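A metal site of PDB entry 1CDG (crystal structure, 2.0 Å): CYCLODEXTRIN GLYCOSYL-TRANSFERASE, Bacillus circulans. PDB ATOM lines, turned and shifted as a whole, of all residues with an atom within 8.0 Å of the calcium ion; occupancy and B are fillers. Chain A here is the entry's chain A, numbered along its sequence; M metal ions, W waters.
The side-chain amide oxygen (OD1) of Asn 29 lies within hydrogen-bond range of the backbone NH (N) of Ala 31 (3.1 Å).
O of Ala 111 sits close to OD1 of Asn 32.
The side-chain carboxylate (OD1) of Asp 53 is in hydrogen-bond range of the backbone NH (N) of Gly 28, at 2.8 Å.
The backbone carbonyl oxygen (O) of Ser 26 is in hydrogen-bond range of the backbone NH (N) of Asp 53, 3.1 Å away.
The backbone NH of Gln 55 sits close to the side-chain carboxylate of Asp 53, 3.3 Å away.
The side-chain carboxylate of Asp 53 lies within hydrogen-bond range of the backbone NH of Gly 56.
OD1 of Asp 23 is in hydrogen-bond range of N of Gly 51.
The calcium ion is bound by OD1 of Asn 33, water W1, O of Asn 29, OD1 of Asn 32, OD2 of Asp 53, OD1 of Asp 27 and O of Gly 51.
The calcium ion has seven donor atoms within binding distance.
Of the 24 residues printed, 6 come within 4 Å of the calcium ion.
The nearest printed residue that does not touch the calcium ion is Pro 30 (4.04 Å).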
ATOM      1  N   THR A  22      13.800   4.582  10.563  1.00  0.00           N
ATOM      2  CA  THR A  22      13.159   4.102  11.773  1.00  0.00           C
ATOM      3  C   THR A  22      14.141   3.707  12.867  1.00  0.00           C
ATOM      4  O   THR A  22      13.912   3.981  14.051  1.00  0.00           O
ATOM      5  CB  THR A  22      12.154   2.937  11.546  1.00  0.00           C
ATOM      6  OG1 THR A  22      11.247   3.221  10.492  1.00  0.00           O
ATOM      7  CG2 THR A  22      11.353   2.593  12.807  1.00  0.00           C
ATOM      8  N   ASP A  23      15.201   3.031  12.473  1.00  0.00           N
ATOM      9  CA  ASP A  23      16.165   2.495  13.409  1.00  0.00           C
ATOM     10  C   ASP A  23      16.944   3.530  14.191  1.00  0.00           C
ATOM     11  O   ASP A  23      17.451   3.321  15.313  1.00  0.00           O
ATOM     12  CB  ASP A  23      17.114   1.535  12.660  1.00  0.00           C
ATOM     13  CG  ASP A  23      18.042   0.860  13.655  1.00  0.00           C
ATOM     14  OD1 ASP A  23      17.571   0.232  14.633  1.00  0.00           O
ATOM     15  OD2 ASP A  23      19.292   1.062  13.422  1.00  0.00           O
ATOM     16  N   SER A  26      13.957   6.746  17.356  1.00  0.00           N
ATOM     17  CA  SER A  26      13.716   6.574  18.789  1.00  0.00           C
ATOM     18  C   SER A  26      13.316   5.138  19.128  1.00  0.00           C
ATOM     19  O   SER A  26      12.347   4.558  18.613  1.00  0.00           O
ATOM     20  CB  SER A  26      12.661   7.565  19.273  1.00  0.00           C
ATOM     21  OG  SER A  26      12.333   7.330  20.643  1.00  0.00           O
ATOM     22  N   ASP A  27      14.077   4.524  20.012  1.00  0.00           N
ATOM     23  CA  ASP A  27      13.810   3.165  20.446  1.00  0.00           C
ATOM     24  C   ASP A  27      12.714   3.155  21.494  1.00  0.00           C
ATOM     25  O   ASP A  27      13.030   3.304  22.643  1.00  0.00           O
ATOM     26  CB  ASP A  27      15.112   2.486  20.979  1.00  0.00           C
ATOM     27  CG  ASP A  27      14.905   1.115  21.573  1.00  0.00           C
ATOM     28  OD1 ASP A  27      13.831   0.484  21.422  1.00  0.00           O
ATOM     29  OD2 ASP A  27      15.934   0.639  22.160  1.00  0.00           O
ATOM     30  N   GLY A  28      11.426   2.983  21.169  1.00  0.00           N
ATOM     31  CA  GLY A  28      10.488   3.030  22.267  1.00  0.00           C
ATOM     32  C   GLY A  28      10.119   1.676  22.830  1.00  0.00           C
ATOM     33  O   GLY A  28       9.294   1.526  23.718  1.00  0.00           O
ATOM     34  N   ASN A  29      10.684   0.667  22.293  1.00  0.00           N
ATOM     35  CA  ASN A  29      10.359  -0.645  22.741  1.00  0.00           C
ATOM     36  C   ASN A  29      11.573  -1.508  22.561  1.00  0.00           C
ATOM     37  O   ASN A  29      11.806  -2.075  21.479  1.00  0.00           O
ATOM     38  CB  ASN A  29       9.151  -1.204  21.995  1.00  0.00           C
ATOM     39  CG  ASN A  29       9.017  -2.690  22.257  1.00  0.00           C
ATOM     40  OD1 ASN A  29       9.469  -3.204  23.294  1.00  0.00           O
ATOM     41  ND2 ASN A  29       8.513  -3.415  21.292  1.00  0.00           N
ATOM     42  N   PRO A  30      12.349  -1.551  23.630  1.00  0.00           N
ATOM     43  CA  PRO A  30      13.620  -2.237  23.750  1.00  0.00           C
ATOM     44  C   PRO A  30      13.488  -3.740  23.657  1.00  0.00           C
ATOM     45  O   PRO A  30      14.435  -4.447  23.332  1.00  0.00           O
ATOM     46  CB  PRO A  30      14.132  -1.913  25.140  1.00  0.00           C
ATOM     47  CG  PRO A  30      12.918  -1.485  25.933  1.00  0.00           C
ATOM     48  CD  PRO A  30      11.832  -1.124  24.938  1.00  0.00           C
ATOM     49  N   ALA A  31      12.291  -4.210  23.913  1.00  0.00           N
ATOM     50  CA  ALA A  31      12.039  -5.629  23.836  1.00  0.00           C
ATOM     51  C   ALA A  31      12.127  -6.212  22.415  1.00  0.00           C
ATOM     52  O   ALA A  31      12.420  -7.389  22.271  1.00  0.00           O
ATOM     53  CB  ALA A  31      10.699  -5.897  24.480  1.00  0.00           C
ATOM     54  N   ASN A  32      11.885  -5.418  21.347  1.00  0.00           N
ATOM     55  CA  ASN A  32      11.983  -5.915  19.968  1.00  0.00           C
ATOM     56  C   ASN A  32      13.346  -5.678  19.356  1.00  0.00           C
ATOM     57  O   ASN A  32      13.503  -5.896  18.169  1.00  0.00           O
ATOM     58  CB  ASN A  32      10.903  -5.369  19.030  1.00  0.00           C
ATOM     59  CG  ASN A  32      10.793  -3.862  19.032  1.00  0.00           C
ATOM     60  OD1 ASN A  32      11.796  -3.185  19.218  1.00  0.00           O
ATOM     61  ND2 ASN A  32       9.577  -3.371  18.880  1.00  0.00           N
ATOM     62  N   ASN A  33      14.325  -5.254  20.162  1.00  0.00           N
ATOM     63  CA  ASN A  33      15.634  -4.968  19.647  1.00  0.00           C
ATOM     64  C   ASN A  33      16.389  -6.211  19.310  1.00  0.00           C
ATOM     65  O   ASN A  33      16.429  -7.116  20.103  1.00  0.00           O
ATOM     66  CB  ASN A  33      16.487  -4.264  20.715  1.00  0.00           C
ATOM     67  CG  ASN A  33      16.027  -2.877  20.961  1.00  0.00           C
ATOM     68  OD1 ASN A  33      15.032  -2.455  20.421  1.00  0.00           O
ATOM     69  ND2 ASN A  33      16.711  -2.166  21.852  1.00  0.00           N
ATOM     70  N   PRO A  34      17.057  -6.227  18.182  1.00  0.00           N
ATOM     71  CA  PRO A  34      17.854  -7.382  17.896  1.00  0.00           C
ATOM     72  C   PRO A  34      18.914  -7.547  18.973  1.00  0.00           C
ATOM     73  O   PRO A  34      19.210  -6.642  19.734  1.00  0.00           O
ATOM     74  CB  PRO A  34      18.419  -7.215  16.498  1.00  0.00           C
ATOM     75  CG  PRO A  34      17.591  -6.116  15.832  1.00  0.00           C
ATOM     76  CD  PRO A  34      16.799  -5.439  16.937  1.00  0.00           C
ATOM     77  N   PHE A  39      23.161  -6.032  17.034  1.00  0.00           N
ATOM     78  CA  PHE A  39      22.769  -4.910  17.778  1.00  0.00           C
ATOM     79  C   PHE A  39      23.913  -4.140  18.436  1.00  0.00           C
ATOM     80  O   PHE A  39      24.905  -4.718  18.864  1.00  0.00           O
ATOM     81  CB  PHE A  39      21.835  -5.446  18.811  1.00  0.00           C
ATOM     82  CG  PHE A  39      21.242  -4.328  19.573  1.00  0.00           C
ATOM     83  CD1 PHE A  39      20.330  -3.454  18.978  1.00  0.00           C
ATOM     84  CD2 PHE A  39      21.509  -4.157  20.925  1.00  0.00           C
ATOM     85  CE1 PHE A  39      19.692  -2.438  19.686  1.00  0.00           C
ATOM     86  CE2 PHE A  39      20.911  -3.109  21.639  1.00  0.00           C
ATOM     87  CZ  PHE A  39      19.998  -2.255  21.029  1.00  0.00           C
ATOM     88  N   TYR A  49      21.968  -2.574  13.974  1.00  0.00           N
ATOM     89  CA  TYR A  49      20.708  -2.053  14.473  1.00  0.00           C
ATOM     90  C   TYR A  49      20.921  -1.265  15.755  1.00  0.00           C
ATOM     91  O   TYR A  49      21.557  -1.770  16.683  1.00  0.00           O
ATOM     92  CB  TYR A  49      19.696  -3.157  14.809  1.00  0.00           C
ATOM     93  CG  TYR A  49      18.860  -3.701  13.657  1.00  0.00           C
ATOM     94  CD1 TYR A  49      17.618  -3.152  13.325  1.00  0.00           C
ATOM     95  CD2 TYR A  49      19.290  -4.842  12.968  1.00  0.00           C
ATOM     96  CE1 TYR A  49      16.830  -3.755  12.353  1.00  0.00           C
ATOM     97  CE2 TYR A  49      18.536  -5.416  11.950  1.00  0.00           C
ATOM     98  CZ  TYR A  49      17.299  -4.858  11.641  1.00  0.00           C
ATOM     99  OH  TYR A  49      16.563  -5.404  10.639  1.00  0.00           O
ATOM    100  N   CYS A  50      20.330  -0.085  15.832  1.00  0.00           N
ATOM    101  CA  CYS A  50      20.431   0.714  17.039  1.00  0.00           C
ATOM    102  C   CYS A  50      19.170   0.597  17.872  1.00  0.00           C
ATOM    103  O   CYS A  50      19.101   0.907  19.058  1.00  0.00           O
ATOM    104  CB  CYS A  50      20.984   2.115  16.820  1.00  0.00           C
ATOM    105  SG  CYS A  50      22.378   2.121  15.715  1.00  0.00           S
ATOM    106  N   GLY A  51      18.137   0.073  17.241  1.00  0.00           N
ATOM    107  CA  GLY A  51      16.922  -0.187  17.964  1.00  0.00           C
ATOM    108  C   GLY A  51      15.713   0.724  17.773  1.00  0.00           C
ATOM    109  O   GLY A  51      14.705   0.488  18.420  1.00  0.00           O
ATOM    110  N   GLY A  52      15.782   1.760  16.916  1.00  0.00           N
ATOM    111  CA  GLY A  52      14.611   2.633  16.766  1.00  0.00           C
ATOM    112  C   GLY A  52      13.437   1.859  16.233  1.00  0.00           C
ATOM    113  O   GLY A  52      13.596   0.963  15.453  1.00  0.00           O
ATOM    114  N   ASP A  53      12.223   2.218  16.605  1.00  0.00           N
ATOM    115  CA  ASP A  53      11.103   1.463  16.105  1.00  0.00           C
ATOM    116  C   ASP A  53       9.813   2.280  15.977  1.00  0.00           C
ATOM    117  O   ASP A  53       9.824   3.463  16.202  1.00  0.00           O
ATOM    118  CB  ASP A  53      10.899   0.358  17.126  1.00  0.00           C
ATOM    119  CG  ASP A  53      10.855   0.925  18.520  1.00  0.00           C
ATOM    120  OD1 ASP A  53      10.331   2.047  18.806  1.00  0.00           O
ATOM    121  OD2 ASP A  53      11.338   0.108  19.366  1.00  0.00           O
ATOM    122  N   TRP A  54       8.679   1.618  15.656  1.00  0.00           N
ATOM    123  CA  TRP A  54       7.412   2.278  15.508  1.00  0.00           C
ATOM    124  C   TRP A  54       6.933   2.855  16.811  1.00  0.00           C
ATOM    125  O   TRP A  54       6.426   3.965  16.834  1.00  0.00           O
ATOM    126  CB  TRP A  54       6.343   1.431  14.807  1.00  0.00           C
ATOM    127  CG  TRP A  54       6.789   1.044  13.430  1.00  0.00           C
ATOM    128  CD1 TRP A  54       7.575   1.781  12.610  1.00  0.00           C
ATOM    129  CD2 TRP A  54       6.494  -0.164  12.717  1.00  0.00           C
ATOM    130  NE1 TRP A  54       7.800   1.129  11.444  1.00  0.00           N
ATOM    131  CE2 TRP A  54       7.160  -0.065  11.462  1.00  0.00           C
ATOM    132  CE3 TRP A  54       5.749  -1.347  13.000  1.00  0.00           C
ATOM    133  CZ2 TRP A  54       7.158  -1.108  10.529  1.00  0.00           C
ATOM    134  CZ3 TRP A  54       5.731  -2.351  12.026  1.00  0.00           C
ATOM    135  CH2 TRP A  54       6.430  -2.238  10.825  1.00  0.00           C
ATOM    136  N   GLN A  55       7.145   2.139  17.911  1.00  0.00           N
ATOM    137  CA  GLN A  55       6.720   2.680  19.192  1.00  0.00           C
ATOM    138  C   GLN A  55       7.399   4.016  19.487  1.00  0.00           C
ATOM    139  O   GLN A  55       6.813   4.974  20.044  1.00  0.00           O
ATOM    140  CB  GLN A  55       7.017   1.696  20.334  1.00  0.00           C
ATOM    141  CG  GLN A  55       6.433   2.187  21.661  1.00  0.00           C
ATOM    142  CD  GLN A  55       4.913   2.235  21.619  1.00  0.00           C
ATOM    143  OE1 GLN A  55       4.221   1.257  21.219  1.00  0.00           O
ATOM    144  NE2 GLN A  55       4.361   3.380  21.984  1.00  0.00           N
ATOM    145  N   GLY A  56       8.672   4.058  19.119  1.00  0.00           N
ATOM    146  CA  GLY A  56       9.487   5.250  19.310  1.00  0.00           C
ATOM    147  C   GLY A  56       8.847   6.434  18.563  1.00  0.00           C
ATOM    148  O   GLY A  56       8.644   7.520  19.125  1.00  0.00           O
ATOM    149  N   PRO A 110      10.360  -7.410  12.368  1.00  0.00           N
ATOM    150  CA  PRO A 110      10.108  -7.398  13.787  1.00  0.00           C
ATOM    151  C   PRO A 110      10.951  -6.405  14.586  1.00  0.00           C
ATOM    152  O   PRO A 110      10.621  -6.078  15.726  1.00  0.00           O
ATOM    153  CB  PRO A 110      10.273  -8.824  14.267  1.00  0.00           C
ATOM    154  CG  PRO A 110      10.966  -9.564  13.120  1.00  0.00           C
ATOM    155  CD  PRO A 110      10.949  -8.680  11.898  1.00  0.00           C
ATOM    156  N   ALA A 111      12.092  -5.961  14.068  1.00  0.00           N
ATOM    157  CA  ALA A 111      12.840  -4.972  14.830  1.00  0.00           C
ATOM    158  C   ALA A 111      12.000  -3.694  14.880  1.00  0.00           C
ATOM    159  O   ALA A 111      12.079  -2.965  15.834  1.00  0.00           O
ATOM    160  CB  ALA A 111      14.199  -4.621  14.257  1.00  0.00           C
ATOM    161  N   TYR A 112      11.223  -3.383  13.848  1.00  0.00           N
ATOM    162  CA  TYR A 112      10.391  -2.179  13.848  1.00  0.00           C
ATOM    163  C   TYR A 112       9.144  -2.392  14.677  1.00  0.00           C
ATOM    164  O   TYR A 112       8.660  -1.508  15.397  1.00  0.00           O
ATOM    165  CB  TYR A 112       9.968  -1.709  12.438  1.00  0.00           C
ATOM    166  CG  TYR A 112      11.131  -1.430  11.547  1.00  0.00           C
ATOM    167  CD1 TYR A 112      12.412  -1.182  12.046  1.00  0.00           C
ATOM    168  CD2 TYR A 112      10.933  -1.421  10.175  1.00  0.00           C
ATOM    169  CE1 TYR A 112      13.501  -0.963  11.194  1.00  0.00           C
ATOM    170  CE2 TYR A 112      12.003  -1.206   9.302  1.00  0.00           C
ATOM    171  CZ  TYR A 112      13.267  -0.948   9.815  1.00  0.00           C
ATOM    172  OH  TYR A 112      14.274  -0.714   8.920  1.00  0.00           O
ATOM    173  N   GLY A 113       8.537  -3.557  14.525  1.00  0.00           N
ATOM    174  CA  GLY A 113       7.324  -3.854  15.301  1.00  0.00           C
ATOM    175  C   GLY A 113       6.446  -4.944  14.705  1.00  0.00           C
ATOM    176  O   GLY A 113       6.776  -5.536  13.685  1.00  0.00           O
HETATM  177 CA    CA M   1      13.347  -1.337  19.716  1.00  0.00          CA
HETATM  178  O   HOH W   1      13.955  -2.329  17.684  1.00  0.00           O
